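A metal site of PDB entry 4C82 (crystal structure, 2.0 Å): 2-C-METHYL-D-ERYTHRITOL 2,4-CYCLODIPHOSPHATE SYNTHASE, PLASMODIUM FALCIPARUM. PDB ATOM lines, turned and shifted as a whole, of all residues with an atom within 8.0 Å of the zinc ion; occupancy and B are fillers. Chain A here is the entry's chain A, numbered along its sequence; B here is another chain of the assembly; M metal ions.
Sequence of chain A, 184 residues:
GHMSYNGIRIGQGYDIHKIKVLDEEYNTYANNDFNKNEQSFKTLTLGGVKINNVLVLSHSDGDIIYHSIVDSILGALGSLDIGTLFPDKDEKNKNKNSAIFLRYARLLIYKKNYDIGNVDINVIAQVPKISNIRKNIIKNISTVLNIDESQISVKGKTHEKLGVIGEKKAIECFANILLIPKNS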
ATOM      1  N   TYR A  14      14.051  24.554 -20.350  1.00  0.00           N
ATOM      2  CA  TYR A  14      13.707  25.726 -19.539  1.00  0.00           C
ATOM      3  C   TYR A  14      12.202  25.886 -19.526  1.00  0.00           C
ATOM      4  O   TYR A  14      11.518  25.647 -20.553  1.00  0.00           O
ATOM      5  CB  TYR A  14      14.382  26.966 -20.213  1.00  0.00           C
ATOM      6  CG  TYR A  14      13.832  28.250 -19.620  1.00  0.00           C
ATOM      7  CD1 TYR A  14      14.356  28.757 -18.477  1.00  0.00           C
ATOM      8  CD2 TYR A  14      12.731  28.909 -20.195  1.00  0.00           C
ATOM      9  CE1 TYR A  14      13.887  29.949 -17.936  1.00  0.00           C
ATOM     10  CE2 TYR A  14      12.230  30.093 -19.655  1.00  0.00           C
ATOM     11  CZ  TYR A  14      12.820  30.619 -18.520  1.00  0.00           C
ATOM     12  OH  TYR A  14      12.345  31.806 -17.883  1.00  0.00           O
ATOM     13  N   ASP A  15      11.637  26.348 -18.404  1.00  0.00           N
ATOM     14  CA  ASP A  15      10.194  26.568 -18.383  1.00  0.00           C
ATOM     15  C   ASP A  15       9.942  27.714 -17.403  1.00  0.00           C
ATOM     16  O   ASP A  15      10.721  27.933 -16.484  1.00  0.00           O
ATOM     17  CB  ASP A  15       9.385  25.330 -17.889  1.00  0.00           C
ATOM     18  CG  ASP A  15       7.884  25.375 -18.336  1.00  0.00           C
ATOM     19  OD1 ASP A  15       7.505  26.232 -19.220  1.00  0.00           O
ATOM     20  OD2 ASP A  15       7.076  24.526 -17.810  1.00  0.00           O
ATOM     21  N   ILE A  16       8.804  28.389 -17.579  1.00  0.00           N
ATOM     22  CA  ILE A  16       8.441  29.463 -16.626  1.00  0.00           C
ATOM     23  C   ILE A  16       6.925  29.480 -16.597  1.00  0.00           C
ATOM     24  O   ILE A  16       6.259  29.354 -17.649  1.00  0.00           O
ATOM     25  CB  ILE A  16       9.065  30.837 -17.020  1.00  0.00           C
ATOM     26  CG1 ILE A  16       8.467  31.981 -16.098  1.00  0.00           C
ATOM     27  CG2 ILE A  16       8.800  31.096 -18.509  1.00  0.00           C
ATOM     28  CD1 ILE A  16       9.140  33.322 -16.304  1.00  0.00           C
ATOM     29  N   HIS A  17       6.349  29.564 -15.393  1.00  0.00           N
ATOM     30  CA  HIS A  17       4.909  29.729 -15.293  1.00  0.00           C
ATOM     31  C   HIS A  17       4.544  30.840 -14.347  1.00  0.00           C
ATOM     32  O   HIS A  17       5.187  31.003 -13.308  1.00  0.00           O
ATOM     33  CB  HIS A  17       4.204  28.434 -14.886  1.00  0.00           C
ATOM     34  CG  HIS A  17       4.036  27.495 -16.031  1.00  0.00           C
ATOM     35  ND1 HIS A  17       3.167  27.729 -17.050  1.00  0.00           N
ATOM     36  CD2 HIS A  17       4.695  26.310 -16.341  1.00  0.00           C
ATOM     37  CE1 HIS A  17       3.271  26.735 -17.947  1.00  0.00           C
ATOM     38  NE2 HIS A  17       4.218  25.871 -17.499  1.00  0.00           N
ATOM     39  N   VAL A  56      -1.373  28.396 -10.103  1.00  0.00           N
ATOM     40  CA  VAL A  56      -0.561  28.544 -11.281  1.00  0.00           C
ATOM     41  C   VAL A  56      -1.582  28.993 -12.327  1.00  0.00           C
ATOM     42  O   VAL A  56      -2.684  28.440 -12.411  1.00  0.00           O
ATOM     43  CB  VAL A  56       0.173  27.215 -11.600  1.00  0.00           C
ATOM     44  CG1 VAL A  56      -0.824  26.100 -11.996  1.00  0.00           C
ATOM     45  CG2 VAL A  56       1.301  27.398 -12.637  1.00  0.00           C
ATOM     46  N   SER A  58      -2.292  29.034 -15.820  1.00  0.00           N
ATOM     47  CA  SER A  58      -1.829  28.283 -16.991  1.00  0.00           C
ATOM     48  C   SER A  58      -2.956  27.426 -17.612  1.00  0.00           C
ATOM     49  O   SER A  58      -3.796  26.877 -16.890  1.00  0.00           O
ATOM     50  CB  SER A  58      -0.701  27.330 -16.556  1.00  0.00           C
ATOM     51  OG  SER A  58       0.287  28.002 -15.781  1.00  0.00           O
ATOM     52  N   SER A  60      -2.032  24.698 -19.055  1.00  0.00           N
ATOM     53  CA  SER A  60      -1.455  23.393 -18.700  1.00  0.00           C
ATOM     54  C   SER A  60      -1.449  23.284 -17.148  1.00  0.00           C
ATOM     55  O   SER A  60      -1.935  24.198 -16.461  1.00  0.00           O
ATOM     56  CB  SER A  60      -0.013  23.310 -19.278  1.00  0.00           C
ATOM     57  OG  SER A  60       0.857  24.199 -18.553  1.00  0.00           O
ATOM     58  N   ASP A  61      -0.916  22.199 -16.588  1.00  0.00           N
ATOM     59  CA  ASP A  61      -0.851  22.004 -15.124  1.00  0.00           C
ATOM     60  C   ASP A  61       0.252  22.848 -14.414  1.00  0.00           C
ATOM     61  O   ASP A  61       0.434  22.788 -13.186  1.00  0.00           O
ATOM     62  CB  ASP A  61      -0.638  20.534 -14.799  1.00  0.00           C
ATOM     63  CG  ASP A  61       0.778  20.037 -15.147  1.00  0.00           C
ATOM     64  OD1 ASP A  61       1.622  20.884 -15.540  1.00  0.00           O
ATOM     65  OD2 ASP A  61       1.055  18.818 -14.989  1.00  0.00           O
ATOM     66  N   GLY A  62       1.055  23.559 -15.200  1.00  0.00           N
ATOM     67  CA  GLY A  62       2.042  24.500 -14.624  1.00  0.00           C
ATOM     68  C   GLY A  62       3.282  23.830 -14.051  1.00  0.00           C
ATOM     69  O   GLY A  62       4.102  24.501 -13.432  1.00  0.00           O
ATOM     70  N   ASP A  63       3.453  22.530 -14.279  1.00  0.00           N
ATOM     71  CA  ASP A  63       4.602  21.789 -13.694  1.00  0.00           C
ATOM     72  C   ASP A  63       5.915  22.116 -14.399  1.00  0.00           C
ATOM     73  O   ASP A  63       6.372  21.360 -15.293  1.00  0.00           O
ATOM     74  CB  ASP A  63       4.273  20.282 -13.614  1.00  0.00           C
ATOM     75  CG  ASP A  63       5.156  19.540 -12.639  1.00  0.00           C
ATOM     76  OD1 ASP A  63       6.337  19.937 -12.511  1.00  0.00           O
ATOM     77  OD2 ASP A  63       4.704  18.594 -11.974  1.00  0.00           O
ATOM     78  N   ILE A  64       6.552  23.235 -13.983  1.00  0.00           N
ATOM     79  CA  ILE A  64       7.798  23.684 -14.620  1.00  0.00           C
ATOM     80  C   ILE A  64       8.841  22.551 -14.563  1.00  0.00           C
ATOM     81  O   ILE A  64       9.677  22.488 -15.390  1.00  0.00           O
ATOM     82  CB  ILE A  64       8.433  24.947 -13.987  1.00  0.00           C
ATOM     83  CG1 ILE A  64       8.476  24.788 -12.436  1.00  0.00           C
ATOM     84  CG2 ILE A  64       7.817  26.259 -14.551  1.00  0.00           C
ATOM     85  CD1 ILE A  64       9.278  25.915 -11.761  1.00  0.00           C
ATOM     86  N   ILE A  65       8.762  21.685 -13.566  1.00  0.00           N
ATOM     87  CA  ILE A  65       9.827  20.673 -13.374  1.00  0.00           C
ATOM     88  C   ILE A  65       9.638  19.550 -14.413  1.00  0.00           C
ATOM     89  O   ILE A  65      10.561  19.249 -15.228  1.00  0.00           O
ATOM     90  CB  ILE A  65       9.881  20.131 -11.937  1.00  0.00           C
ATOM     91  CG1 ILE A  65      10.500  21.150 -10.965  1.00  0.00           C
ATOM     92  CG2 ILE A  65      10.813  18.858 -11.834  1.00  0.00           C
ATOM     93  CD1 ILE A  65      10.611  20.603  -9.516  1.00  0.00           C
ATOM     94  N   TYR A  66       8.425  18.940 -14.405  1.00  0.00           N
ATOM     95  CA  TYR A  66       8.100  18.017 -15.516  1.00  0.00           C
ATOM     96  C   TYR A  66       8.260  18.569 -16.905  1.00  0.00           C
ATOM     97  O   TYR A  66       8.812  17.886 -17.766  1.00  0.00           O
ATOM     98  CB  TYR A  66       6.683  17.420 -15.343  1.00  0.00           C
ATOM     99  CG  TYR A  66       6.609  16.372 -14.244  1.00  0.00           C
ATOM    100  CD1 TYR A  66       7.776  15.894 -13.609  1.00  0.00           C
ATOM    101  CD2 TYR A  66       5.371  15.784 -13.920  1.00  0.00           C
ATOM    102  CE1 TYR A  66       7.694  14.897 -12.624  1.00  0.00           C
ATOM    103  CE2 TYR A  66       5.258  14.774 -12.959  1.00  0.00           C
ATOM    104  CZ  TYR A  66       6.408  14.341 -12.310  1.00  0.00           C
ATOM    105  OH  TYR A  66       6.241  13.365 -11.371  1.00  0.00           O
ATOM    106  N   HIS A  67       7.796  19.796 -17.163  1.00  0.00           N
ATOM    107  CA  HIS A  67       7.925  20.308 -18.520  1.00  0.00           C
ATOM    108  C   HIS A  67       9.349  20.583 -18.862  1.00  0.00           C
ATOM    109  O   HIS A  67       9.715  20.361 -19.989  1.00  0.00           O
ATOM    110  CB  HIS A  67       7.100  21.595 -18.791  1.00  0.00           C
ATOM    111  CG  HIS A  67       5.672  21.508 -18.349  1.00  0.00           C
ATOM    112  ND1 HIS A  67       4.861  22.602 -18.318  1.00  0.00           N
ATOM    113  CD2 HIS A  67       4.882  20.381 -17.959  1.00  0.00           C
ATOM    114  CE1 HIS A  67       3.607  22.208 -17.904  1.00  0.00           C
ATOM    115  NE2 HIS A  67       3.640  20.850 -17.645  1.00  0.00           N
ATOM    116  N   SER A  68      10.196  21.041 -17.924  1.00  0.00           N
ATOM    117  CA  SER A  68      11.556  21.395 -18.393  1.00  0.00           C
ATOM    118  C   SER A  68      12.320  20.088 -18.594  1.00  0.00           C
ATOM    119  O   SER A  68      13.171  19.979 -19.481  1.00  0.00           O
ATOM    120  CB  SER A  68      12.314  22.350 -17.446  1.00  0.00           C
ATOM    121  OG  SER A  68      12.487  21.746 -16.228  1.00  0.00           O
ATOM    122  N   ASP A  71      11.546  18.978 -21.966  1.00  0.00           N
ATOM    123  CA  ASP A  71      12.208  19.801 -22.954  1.00  0.00           C
ATOM    124  C   ASP A  71      13.704  19.542 -23.023  1.00  0.00           C
ATOM    125  O   ASP A  71      14.268  19.702 -24.093  1.00  0.00           O
ATOM    126  CB  ASP A  71      11.925  21.300 -22.693  1.00  0.00           C
ATOM    127  CG  ASP A  71      10.718  21.800 -23.496  1.00  0.00           C
ATOM    128  OD1 ASP A  71      10.024  20.974 -24.149  1.00  0.00           O
ATOM    129  OD2 ASP A  71      10.497  23.021 -23.493  1.00  0.00           O
ATOM    130  N   ILE A  82       7.149  20.004 -27.269  1.00  0.00           N
ATOM    131  CA  ILE A  82       5.839  19.419 -26.896  1.00  0.00           C
ATOM    132  C   ILE A  82       4.618  20.014 -27.640  1.00  0.00           C
ATOM    133  O   ILE A  82       3.833  19.292 -28.306  1.00  0.00           O
ATOM    134  CB  ILE A  82       5.706  19.430 -25.351  1.00  0.00           C
ATOM    135  CG1 ILE A  82       6.306  18.132 -24.741  1.00  0.00           C
ATOM    136  CG2 ILE A  82       4.276  19.703 -24.868  1.00  0.00           C
ATOM    137  CD1 ILE A  82       6.061  16.842 -25.508  1.00  0.00           C
ATOM    138  N   SER A  98       0.994  16.290 -18.489  1.00  0.00           N
ATOM    139  CA  SER A  98       2.427  16.196 -18.102  1.00  0.00           C
ATOM    140  C   SER A  98       2.938  14.778 -18.058  1.00  0.00           C
ATOM    141  O   SER A  98       4.104  14.551 -18.411  1.00  0.00           O
ATOM    142  CB  SER A  98       2.831  16.982 -16.838  1.00  0.00           C
ATOM    143  OG  SER A  98       2.489  18.366 -16.953  1.00  0.00           O
ATOM    144  N   LYS B 157      10.982  29.819 -26.123  1.00  0.00           N
ATOM    145  CA  LYS B 157      10.123  29.818 -24.973  1.00  0.00           C
ATOM    146  C   LYS B 157       9.717  31.211 -24.777  1.00  0.00           C
ATOM    147  O   LYS B 157      10.569  32.067 -24.730  1.00  0.00           O
ATOM    148  CB  LYS B 157      10.893  29.363 -23.716  1.00  0.00           C
ATOM    149  CG  LYS B 157      10.942  27.797 -23.586  1.00  0.00           C
ATOM    150  CD  LYS B 157       9.543  27.233 -23.226  1.00  0.00           C
ATOM    151  CE  LYS B 157       8.832  28.085 -22.145  1.00  0.00           C
ATOM    152  NZ  LYS B 157       7.580  27.465 -21.604  1.00  0.00           N
ATOM    153  N   GLU B 160       5.646  34.589 -20.534  1.00  0.00           N
ATOM    154  CA  GLU B 160       4.410  34.892 -19.720  1.00  0.00           C
ATOM    155  C   GLU B 160       4.031  36.374 -19.703  1.00  0.00           C
ATOM    156  O   GLU B 160       3.325  36.854 -18.789  1.00  0.00           O
ATOM    157  CB  GLU B 160       4.600  34.351 -18.293  1.00  0.00           C
ATOM    158  CG  GLU B 160       4.867  32.824 -18.257  1.00  0.00           C
ATOM    159  CD  GLU B 160       3.583  32.046 -18.595  1.00  0.00           C
ATOM    160  OE1 GLU B 160       2.646  32.090 -17.792  1.00  0.00           O
ATOM    161  OE2 GLU B 160       3.489  31.419 -19.656  1.00  0.00           O
HETATM  162 ZN    ZN M   1       5.253  24.530 -18.660  1.00  0.00          ZN
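The side-chain carboxylate (OD1) of Asp 61 sits at hydrogen-bond distance from a ring nitrogen (NE2) of His 67. OG of Ser 58 sits at hydrogen-bond distance from ND1 of His 17. OD1 of Asp 15 lies within salt-bridge range of NZ of Lys 157 of chain B, 2.7 Å away. NE2 of His 67 lies within hydrogen-bond range of OG of Ser 98 (2.8 Å).
The zinc ion is bound by a ring nitrogen (ND1) of His 67 (2.0 Å), the side-chain carboxylate (OD2) of Asp 15 (2.0 Å) and a ring nitrogen (NE2) of His 17 (2.1 Å). The zinc ion has three donor atoms within binding distance.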
